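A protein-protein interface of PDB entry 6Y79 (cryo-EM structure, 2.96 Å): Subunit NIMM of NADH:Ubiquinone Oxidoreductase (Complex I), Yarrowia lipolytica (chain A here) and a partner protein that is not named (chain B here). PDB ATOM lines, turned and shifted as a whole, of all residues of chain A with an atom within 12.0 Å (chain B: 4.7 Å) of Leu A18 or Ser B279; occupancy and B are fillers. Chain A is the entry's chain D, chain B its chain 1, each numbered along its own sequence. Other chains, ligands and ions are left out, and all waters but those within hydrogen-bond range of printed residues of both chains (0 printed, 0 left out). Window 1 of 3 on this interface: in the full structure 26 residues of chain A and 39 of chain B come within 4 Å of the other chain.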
ATOM      1  N   LEU A   9      -2.977  34.566   6.999  1.00  0.00           N
ATOM      2  CA  LEU A   9      -2.632  33.605   5.963  1.00  0.00           C
ATOM      3  C   LEU A   9      -3.123  32.178   6.238  1.00  0.00           C
ATOM      4  O   LEU A   9      -3.671  31.601   5.296  1.00  0.00           O
ATOM      5  CB  LEU A   9      -1.134  33.655   5.647  1.00  0.00           C
ATOM      6  CG  LEU A   9      -0.929  34.805   4.652  1.00  0.00           C
ATOM      7  CD1 LEU A   9       0.556  35.133   4.411  1.00  0.00           C
ATOM      8  CD2 LEU A   9      -1.791  34.712   3.268  1.00  0.00           C
ATOM      9  N   PRO A  10      -3.016  31.573   7.444  1.00  0.00           N
ATOM     10  CA  PRO A  10      -3.622  30.237   7.624  1.00  0.00           C
ATOM     11  C   PRO A  10      -5.128  30.219   7.480  1.00  0.00           C
ATOM     12  O   PRO A  10      -5.678  29.211   7.021  1.00  0.00           O
ATOM     13  CB  PRO A  10      -3.201  29.849   9.044  1.00  0.00           C
ATOM     14  CG  PRO A  10      -2.023  30.630   9.303  1.00  0.00           C
ATOM     15  CD  PRO A  10      -2.241  31.923   8.648  1.00  0.00           C
ATOM     16  N   TYR A  11      -5.803  31.319   7.816  1.00  0.00           N
ATOM     17  CA  TYR A  11      -7.187  31.500   7.397  1.00  0.00           C
ATOM     18  C   TYR A  11      -7.303  31.566   5.888  1.00  0.00           C
ATOM     19  O   TYR A  11      -8.290  31.091   5.324  1.00  0.00           O
ATOM     20  CB  TYR A  11      -7.760  32.772   7.993  1.00  0.00           C
ATOM     21  CG  TYR A  11      -7.921  32.693   9.463  1.00  0.00           C
ATOM     22  CD1 TYR A  11      -9.003  32.032  10.025  1.00  0.00           C
ATOM     23  CD2 TYR A  11      -6.994  33.263  10.293  1.00  0.00           C
ATOM     24  CE1 TYR A  11      -9.149  31.952  11.384  1.00  0.00           C
ATOM     25  CE2 TYR A  11      -7.132  33.189  11.628  1.00  0.00           C
ATOM     26  CZ  TYR A  11      -8.203  32.541  12.179  1.00  0.00           C
ATOM     27  OH  TYR A  11      -8.316  32.487  13.536  1.00  0.00           O
ATOM     28  N   GLY A  12      -6.313  32.164   5.223  1.00  0.00           N
ATOM     29  CA  GLY A  12      -6.327  32.204   3.774  1.00  0.00           C
ATOM     30  C   GLY A  12      -6.213  30.829   3.153  1.00  0.00           C
ATOM     31  O   GLY A  12      -6.868  30.534   2.153  1.00  0.00           O
ATOM     32  N   ILE A  13      -5.421  29.950   3.764  1.00  0.00           N
ATOM     33  CA  ILE A  13      -5.288  28.602   3.228  1.00  0.00           C
ATOM     34  C   ILE A  13      -6.515  27.765   3.579  1.00  0.00           C
ATOM     35  O   ILE A  13      -6.968  26.962   2.762  1.00  0.00           O
ATOM     36  CB  ILE A  13      -3.956  27.951   3.665  1.00  0.00           C
ATOM     37  CG1 ILE A  13      -2.760  28.574   2.934  1.00  0.00           C
ATOM     38  CG2 ILE A  13      -3.898  26.470   3.359  1.00  0.00           C
ATOM     39  CD1 ILE A  13      -1.858  29.425   3.767  1.00  0.00           C
ATOM     40  N   ILE A  14      -7.109  27.975   4.765  1.00  0.00           N
ATOM     41  CA  ILE A  14      -8.382  27.318   5.100  1.00  0.00           C
ATOM     42  C   ILE A  14      -9.473  27.711   4.105  1.00  0.00           C
ATOM     43  O   ILE A  14     -10.186  26.852   3.555  1.00  0.00           O
ATOM     44  CB  ILE A  14      -8.801  27.659   6.543  1.00  0.00           C
ATOM     45  CG1 ILE A  14      -7.922  26.945   7.559  1.00  0.00           C
ATOM     46  CG2 ILE A  14     -10.234  27.253   6.805  1.00  0.00           C
ATOM     47  CD1 ILE A  14      -8.012  27.561   8.932  1.00  0.00           C
ATOM     48  N   PHE A  15      -9.565  29.010   3.816  1.00  0.00           N
ATOM     49  CA  PHE A  15     -10.510  29.546   2.845  1.00  0.00           C
ATOM     50  C   PHE A  15     -10.258  28.987   1.449  1.00  0.00           C
ATOM     51  O   PHE A  15     -11.193  28.573   0.757  1.00  0.00           O
ATOM     52  CB  PHE A  15     -10.393  31.069   2.857  1.00  0.00           C
ATOM     53  CG  PHE A  15     -11.276  31.762   1.880  1.00  0.00           C
ATOM     54  CD1 PHE A  15     -12.620  31.915   2.140  1.00  0.00           C
ATOM     55  CD2 PHE A  15     -10.755  32.290   0.714  1.00  0.00           C
ATOM     56  CE1 PHE A  15     -13.435  32.565   1.248  1.00  0.00           C
ATOM     57  CE2 PHE A  15     -11.566  32.940  -0.186  1.00  0.00           C
ATOM     58  CZ  PHE A  15     -12.908  33.078   0.082  1.00  0.00           C
ATOM     59  N   GLY A  16      -8.991  28.924   1.039  1.00  0.00           N
ATOM     60  CA  GLY A  16      -8.673  28.431  -0.289  1.00  0.00           C
ATOM     61  C   GLY A  16      -8.891  26.939  -0.442  1.00  0.00           C
ATOM     62  O   GLY A  16      -9.341  26.483  -1.495  1.00  0.00           O
ATOM     63  N   LEU A  17      -8.596  26.165   0.605  1.00  0.00           N
ATOM     64  CA  LEU A  17      -8.804  24.721   0.556  1.00  0.00           C
ATOM     65  C   LEU A  17     -10.283  24.384   0.480  1.00  0.00           C
ATOM     66  O   LEU A  17     -10.687  23.551  -0.339  1.00  0.00           O
ATOM     67  CB  LEU A  17      -8.176  24.046   1.771  1.00  0.00           C
ATOM     68  CG  LEU A  17      -6.658  23.902   1.811  1.00  0.00           C
ATOM     69  CD1 LEU A  17      -6.239  23.543   3.217  1.00  0.00           C
ATOM     70  CD2 LEU A  17      -6.156  22.886   0.803  1.00  0.00           C
ATOM     71  N   LEU A  18     -11.113  25.053   1.291  1.00  0.00           N
ATOM     72  CA  LEU A  18     -12.546  24.783   1.224  1.00  0.00           C
ATOM     73  C   LEU A  18     -13.167  25.307  -0.068  1.00  0.00           C
ATOM     74  O   LEU A  18     -14.060  24.656  -0.626  1.00  0.00           O
ATOM     75  CB  LEU A  18     -13.245  25.367   2.444  1.00  0.00           C
ATOM     76  CG  LEU A  18     -12.841  24.668   3.739  1.00  0.00           C
ATOM     77  CD1 LEU A  18     -13.322  25.436   4.931  1.00  0.00           C
ATOM     78  CD2 LEU A  18     -13.379  23.255   3.764  1.00  0.00           C
ATOM     79  N   THR A  19     -12.667  26.435  -0.587  1.00  0.00           N
ATOM     80  CA  THR A  19     -13.154  26.978  -1.852  1.00  0.00           C
ATOM     81  C   THR A  19     -12.829  26.055  -3.022  1.00  0.00           C
ATOM     82  O   THR A  19     -13.705  25.742  -3.845  1.00  0.00           O
ATOM     83  CB  THR A  19     -12.538  28.357  -2.072  1.00  0.00           C
ATOM     84  OG1 THR A  19     -12.966  29.239  -1.030  1.00  0.00           O
ATOM     85  CG2 THR A  19     -12.952  28.928  -3.402  1.00  0.00           C
ATOM     86  N   ALA A  20     -11.574  25.601  -3.104  1.00  0.00           N
ATOM     87  CA  ALA A  20     -11.173  24.704  -4.177  1.00  0.00           C
ATOM     88  C   ALA A  20     -11.852  23.351  -4.053  1.00  0.00           C
ATOM     89  O   ALA A  20     -12.190  22.737  -5.074  1.00  0.00           O
ATOM     90  CB  ALA A  20      -9.656  24.543  -4.182  1.00  0.00           C
ATOM     91  N   GLY A  21     -12.098  22.893  -2.822  1.00  0.00           N
ATOM     92  CA  GLY A  21     -12.815  21.643  -2.637  1.00  0.00           C
ATOM     93  C   GLY A  21     -14.249  21.719  -3.117  1.00  0.00           C
ATOM     94  O   GLY A  21     -14.725  20.823  -3.816  1.00  0.00           O
ATOM     95  N   GLY A  22     -14.943  22.810  -2.776  1.00  0.00           N
ATOM     96  CA  GLY A  22     -16.308  22.984  -3.247  1.00  0.00           C
ATOM     97  C   GLY A  22     -16.412  23.128  -4.754  1.00  0.00           C
ATOM     98  O   GLY A  22     -17.315  22.558  -5.375  1.00  0.00           O
ATOM     99  N   GLY A  23     -15.469  23.850  -5.369  1.00  0.00           N
ATOM    100  CA  GLY A  23     -15.506  24.010  -6.817  1.00  0.00           C
ATOM    101  C   GLY A  23     -15.217  22.720  -7.564  1.00  0.00           C
ATOM    102  O   GLY A  23     -15.926  22.363  -8.523  1.00  0.00           O
ATOM    103  N   ALA A  24     -14.176  21.996  -7.129  1.00  0.00           N
ATOM    104  CA  ALA A  24     -13.845  20.715  -7.739  1.00  0.00           C
ATOM    105  C   ALA A  24     -14.968  19.708  -7.551  1.00  0.00           C
ATOM    106  O   ALA A  24     -15.277  18.934  -8.464  1.00  0.00           O
ATOM    107  CB  ALA A  24     -12.544  20.178  -7.149  1.00  0.00           C
ATOM    108  N   MET A  25     -15.641  19.756  -6.401  1.00  0.00           N
ATOM    109  CA  MET A  25     -16.728  18.825  -6.145  1.00  0.00           C
ATOM    110  C   MET A  25     -17.959  19.146  -6.987  1.00  0.00           C
ATOM    111  O   MET A  25     -18.644  18.228  -7.454  1.00  0.00           O
ATOM    112  CB  MET A  25     -17.053  18.826  -4.657  1.00  0.00           C
ATOM    113  CG  MET A  25     -16.210  17.873  -3.842  1.00  0.00           C
ATOM    114  SD  MET A  25     -16.403  18.179  -2.083  1.00  0.00           S
ATOM    115  CE  MET A  25     -17.895  17.250  -1.742  1.00  0.00           C
ATOM    116  N   GLN A  26     -18.250  20.437  -7.212  1.00  0.00           N
ATOM    117  CA  GLN A  26     -19.357  20.803  -8.101  1.00  0.00           C
ATOM    118  C   GLN A  26     -19.109  20.335  -9.529  1.00  0.00           C
ATOM    119  O   GLN A  26     -20.025  19.824 -10.188  1.00  0.00           O
ATOM    120  CB  GLN A  26     -19.589  22.315  -8.090  1.00  0.00           C
ATOM    121  CG  GLN A  26     -20.588  22.834  -9.141  1.00  0.00           C
ATOM    122  CD  GLN A  26     -22.058  22.596  -8.804  1.00  0.00           C
ATOM    123  OE1 GLN A  26     -22.512  22.880  -7.707  1.00  0.00           O
ATOM    124  NE2 GLN A  26     -22.809  22.101  -9.769  1.00  0.00           N
ATOM    125  N   VAL A  27     -17.873  20.473 -10.018  1.00  0.00           N
ATOM    126  CA  VAL A  27     -17.599  20.023 -11.384  1.00  0.00           C
ATOM    127  C   VAL A  27     -17.619  18.498 -11.470  1.00  0.00           C
ATOM    128  O   VAL A  27     -18.070  17.929 -12.472  1.00  0.00           O
ATOM    129  CB  VAL A  27     -16.283  20.641 -11.893  1.00  0.00           C
ATOM    130  CG1 VAL A  27     -15.760  19.971 -13.156  1.00  0.00           C
ATOM    131  CG2 VAL A  27     -16.539  22.062 -12.216  1.00  0.00           C
ATOM    132  N   LEU A  28     -17.216  17.811 -10.394  1.00  0.00           N
ATOM    133  CA  LEU A  28     -17.337  16.352 -10.361  1.00  0.00           C
ATOM    134  C   LEU A  28     -18.796  15.901 -10.388  1.00  0.00           C
ATOM    135  O   LEU A  28     -19.138  14.927 -11.071  1.00  0.00           O
ATOM    136  CB  LEU A  28     -16.627  15.800  -9.129  1.00  0.00           C
ATOM    137  CG  LEU A  28     -15.102  15.744  -9.215  1.00  0.00           C
ATOM    138  CD1 LEU A  28     -14.505  15.251  -7.918  1.00  0.00           C
ATOM    139  CD2 LEU A  28     -14.662  14.875 -10.373  1.00  0.00           C
ATOM    140  N   HIS A  29     -19.674  16.627  -9.691  1.00  0.00           N
ATOM    141  CA  HIS A  29     -21.101  16.310  -9.718  1.00  0.00           C
ATOM    142  C   HIS A  29     -21.708  16.546 -11.094  1.00  0.00           C
ATOM    143  O   HIS A  29     -22.526  15.746 -11.565  1.00  0.00           O
ATOM    144  CB  HIS A  29     -21.841  17.148  -8.683  1.00  0.00           C
ATOM    145  CG  HIS A  29     -21.746  16.614  -7.292  1.00  0.00           C
ATOM    146  ND1 HIS A  29     -22.286  15.403  -6.919  1.00  0.00           N
ATOM    147  CD2 HIS A  29     -21.183  17.132  -6.179  1.00  0.00           C
ATOM    148  CE1 HIS A  29     -22.049  15.196  -5.638  1.00  0.00           C
ATOM    149  NE2 HIS A  29     -21.378  16.229  -5.165  1.00  0.00           N
ATOM    150  N   VAL B  15     -10.759  18.678   4.099  1.00  0.00           N
ATOM    151  CA  VAL B  15     -11.186  18.932   5.473  1.00  0.00           C
ATOM    152  C   VAL B  15     -10.111  18.520   6.474  1.00  0.00           C
ATOM    153  O   VAL B  15      -9.942  19.172   7.512  1.00  0.00           O
ATOM    154  CB  VAL B  15     -12.551  18.278   5.770  1.00  0.00           C
ATOM    155  CG1 VAL B  15     -13.583  18.811   4.806  1.00  0.00           C
ATOM    156  CG2 VAL B  15     -12.497  16.761   5.716  1.00  0.00           C
ATOM    157  N   SER B  18      -7.670  21.317   6.503  1.00  0.00           N
ATOM    158  CA  SER B  18      -8.183  22.543   7.103  1.00  0.00           C
ATOM    159  C   SER B  18      -8.365  22.437   8.610  1.00  0.00           C
ATOM    160  O   SER B  18      -8.388  23.469   9.287  1.00  0.00           O
ATOM    161  CB  SER B  18      -9.504  22.933   6.452  1.00  0.00           C
ATOM    162  OG  SER B  18     -10.514  22.002   6.776  1.00  0.00           O
ATOM    163  N   LEU B  93     -21.414  22.116   0.278  1.00  0.00           N
ATOM    164  CA  LEU B  93     -20.608  23.178  -0.308  1.00  0.00           C
ATOM    165  C   LEU B  93     -21.230  23.691  -1.591  1.00  0.00           C
ATOM    166  O   LEU B  93     -20.525  23.916  -2.570  1.00  0.00           O
ATOM    167  CB  LEU B  93     -19.204  22.656  -0.578  1.00  0.00           C
ATOM    168  CG  LEU B  93     -18.422  22.046   0.584  1.00  0.00           C
ATOM    169  CD1 LEU B  93     -17.339  21.134   0.060  1.00  0.00           C
ATOM    170  CD2 LEU B  93     -17.814  23.140   1.418  1.00  0.00           C
ATOM    171  N   GLY B 275     -19.409  26.954  -8.456  1.00  0.00           N
ATOM    172  CA  GLY B 275     -18.979  26.246  -7.264  1.00  0.00           C
ATOM    173  C   GLY B 275     -17.941  27.003  -6.464  1.00  0.00           C
ATOM    174  O   GLY B 275     -17.955  26.953  -5.228  1.00  0.00           O
ATOM    175  N   LEU B 276     -17.052  27.731  -7.154  1.00  0.00           N
ATOM    176  CA  LEU B 276     -16.095  28.598  -6.473  1.00  0.00           C
ATOM    177  C   LEU B 276     -16.801  29.682  -5.671  1.00  0.00           C
ATOM    178  O   LEU B 276     -16.454  29.915  -4.508  1.00  0.00           O
ATOM    179  CB  LEU B 276     -15.145  29.236  -7.485  1.00  0.00           C
ATOM    180  CG  LEU B 276     -13.970  28.441  -8.048  1.00  0.00           C
ATOM    181  CD1 LEU B 276     -13.125  29.348  -8.923  1.00  0.00           C
ATOM    182  CD2 LEU B 276     -13.143  27.816  -6.950  1.00  0.00           C
ATOM    183  N   ILE B 277     -17.824  30.316  -6.257  1.00  0.00           N
ATOM    184  CA  ILE B 277     -18.545  31.383  -5.557  1.00  0.00           C
ATOM    185  C   ILE B 277     -19.316  30.832  -4.358  1.00  0.00           C
ATOM    186  O   ILE B 277     -19.275  31.405  -3.257  1.00  0.00           O
ATOM    187  CB  ILE B 277     -19.475  32.137  -6.524  1.00  0.00           C
ATOM    188  CG1 ILE B 277     -18.672  32.820  -7.621  1.00  0.00           C
ATOM    189  CG2 ILE B 277     -20.250  33.203  -5.794  1.00  0.00           C
ATOM    190  CD1 ILE B 277     -19.530  33.464  -8.673  1.00  0.00           C
ATOM    191  N   ASN B 278     -19.983  29.686  -4.540  1.00  0.00           N
ATOM    192  CA  ASN B 278     -20.797  29.107  -3.473  1.00  0.00           C
ATOM    193  C   ASN B 278     -19.946  28.656  -2.293  1.00  0.00           C
ATOM    194  O   ASN B 278     -20.214  29.031  -1.142  1.00  0.00           O
ATOM    195  CB  ASN B 278     -21.615  27.939  -4.012  1.00  0.00           C
ATOM    196  CG  ASN B 278     -22.750  28.390  -4.888  1.00  0.00           C
ATOM    197  OD1 ASN B 278     -23.310  29.461  -4.685  1.00  0.00           O
ATOM    198  ND2 ASN B 278     -23.101  27.573  -5.865  1.00  0.00           N
ATOM    199  N   SER B 279     -18.898  27.874  -2.548  1.00  0.00           N
ATOM    200  CA  SER B 279     -18.101  27.432  -1.418  1.00  0.00           C
ATOM    201  C   SER B 279     -17.179  28.527  -0.886  1.00  0.00           C
ATOM    202  O   SER B 279     -16.737  28.421   0.254  1.00  0.00           O
ATOM    203  CB  SER B 279     -17.313  26.181  -1.775  1.00  0.00           C
ATOM    204  OG  SER B 279     -16.345  26.443  -2.761  1.00  0.00           O
ATOM    205  N   SER B 280     -16.926  29.603  -1.640  1.00  0.00           N
ATOM    206  CA  SER B 280     -16.228  30.758  -1.077  1.00  0.00           C
ATOM    207  C   SER B 280     -17.099  31.498  -0.077  1.00  0.00           C
ATOM    208  O   SER B 280     -16.601  31.978   0.951  1.00  0.00           O
ATOM    209  CB  SER B 280     -15.794  31.708  -2.193  1.00  0.00           C
ATOM    210  OG  SER B 280     -16.909  32.312  -2.823  1.00  0.00           O
ATOM    211  N   ALA B 281     -18.405  31.598  -0.369  1.00  0.00           N
ATOM    212  CA  ALA B 281     -19.341  32.162   0.601  1.00  0.00           C
ATOM    213  C   ALA B 281     -19.450  31.292   1.850  1.00  0.00           C
ATOM    214  O   ALA B 281     -19.413  31.800   2.982  1.00  0.00           O
ATOM    215  CB  ALA B 281     -20.701  32.336  -0.049  1.00  0.00           C
ATOM    216  N   TYR B 282     -19.554  29.975   1.661  1.00  0.00           N
ATOM    217  CA  TYR B 282     -19.635  29.054   2.794  1.00  0.00           C
ATOM    218  C   TYR B 282     -18.369  29.094   3.641  1.00  0.00           C
ATOM    219  O   TYR B 282     -18.436  29.183   4.877  1.00  0.00           O
ATOM    220  CB  TYR B 282     -19.901  27.644   2.271  1.00  0.00           C
ATOM    221  CG  TYR B 282     -20.072  26.568   3.313  1.00  0.00           C
ATOM    222  CD1 TYR B 282     -21.276  26.400   3.983  1.00  0.00           C
ATOM    223  CD2 TYR B 282     -19.040  25.697   3.599  1.00  0.00           C
ATOM    224  CE1 TYR B 282     -21.443  25.417   4.919  1.00  0.00           C
ATOM    225  CE2 TYR B 282     -19.191  24.698   4.532  1.00  0.00           C
ATOM    226  CZ  TYR B 282     -20.398  24.567   5.189  1.00  0.00           C
ATOM    227  OH  TYR B 282     -20.558  23.574   6.118  1.00  0.00           O
ATOM    228  N   ALA B 283     -17.204  29.097   2.988  1.00  0.00           N
ATOM    229  CA  ALA B 283     -15.935  29.136   3.695  1.00  0.00           C
ATOM    230  C   ALA B 283     -15.709  30.473   4.383  1.00  0.00           C
ATOM    231  O   ALA B 283     -15.095  30.504   5.440  1.00  0.00           O
ATOM    232  CB  ALA B 283     -14.786  28.845   2.733  1.00  0.00           C
ATOM    233  N   LEU B 286     -17.655  30.322   7.597  1.00  0.00           N
ATOM    234  CA  LEU B 286     -16.993  29.395   8.506  1.00  0.00           C
ATOM    235  C   LEU B 286     -15.702  29.971   9.083  1.00  0.00           C
ATOM    236  O   LEU B 286     -15.421  29.790  10.273  1.00  0.00           O
ATOM    237  CB  LEU B 286     -16.753  28.101   7.739  1.00  0.00           C
ATOM    238  CG  LEU B 286     -16.228  26.789   8.268  1.00  0.00           C
ATOM    239  CD1 LEU B 286     -16.924  25.687   7.496  1.00  0.00           C
ATOM    240  CD2 LEU B 286     -14.746  26.769   8.012  1.00  0.00           C
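O of Thr A19 lies within hydrogen-bond range of OG of Ser B279 (2.9 Å).
The backbone carbonyl oxygen (O) of Val B15 is in hydrogen-bond range of the side-chain hydroxyl (OG) of Ser B18 (3.0 Å).
The side-chain hydroxyl (OG) of Ser B279 sits at hydrogen-bond distance from the backbone carbonyl oxygen (O) of Gly B275, 3.0 Å away.
The backbone carbonyl oxygen of Leu B276 sits at hydrogen-bond distance from the side-chain hydroxyl of Ser B280, at 3.0 Å.
The backbone carbonyl oxygen of Ile B277 sits at hydrogen-bond distance from the side-chain hydroxyl of Ser B280.
O of Phe A15 is in hydrogen-bond range of OG1 of Thr A19, 2.6 Å away.
Ile A14 touches Ser B18.
Phe A15 touches Ser B280 (CE1 to O, 3.2 Å).
Ala B283 touches Phe A15.
Leu A18 touches Ser B279 (O to OG, 3.6 Å).
Leu A18 touches Ala B283.
CG2 of Thr A19 touches CD2 of Leu B276, at 3.7 Å.
Gly A22 touches Leu B93 (CA to CD1, 3.9 Å).
Gly A22 touches Ser B279.
N of Gly A23 touches OG of Ser B279, at 3.8 Å.
SD of Met A25 touches CD1 of Leu B93 (3.8 Å).
Gly A12 touches none of the printed residues of chain B.
Of the printed residues of chain B, Ile A14 touches Ser B18.
Of the printed residues of chain B, Phe A15 touches Ser B280 (3.2 Å) and Ala B283 (3.8 Å).
Leu A18 touches three residues of chain B.
Of the printed residues of chain B, Thr A19 touches Leu B276 (3.7 Å), Ser B279 (2.9 Å) and Ser B280 (3.6 Å).
Printed residues of chain B within 4 Å of Met A25: Leu B93 (3.8 Å).
Gln A26 touches none of the printed residues of chain B.
Ser B18 touches just one residue of chain A: Ile A14 (3.9 Å).
Leu B93 touches just these residues of chain A: Gly A22 (3.9 Å) and Met A25 (3.8 Å).
Of the printed residues of chain A, Leu B276 touches Thr A19 (3.7 Å).
No residue of chain A comes within 4 Å of Asn B278.
Ser B279 touches just these residues of chain A: Leu A18, Thr A19, Gly A22 and Gly A23.
Ser B280 touches two residues of chain A.
No residue of chain A comes within 4 Å of Ala B281.
Ala B283 touches just these residues of chain A: Phe A15 and Leu A18.
Leu B286 touches just one residue of chain A: Leu A18 (3.6 Å).
The nearest residue of chain B that does not touch Leu A18 is Ser B18 (4.3 Å).
Hydrophobic or aromatic side chains of chain B that line the printed part of chain A: Leu B93, Leu B276, Ala B283 and Leu B286.
Of the 21 printed residues of chain A, 7 touch a printed residue of chain B.
Among the printed residues, 14 pairs touch across the chains.
Among the printed residues, no Asp or Glu carboxylate lies within 4 Å of a Lys or Arg side-chain nitrogen of the other chain.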
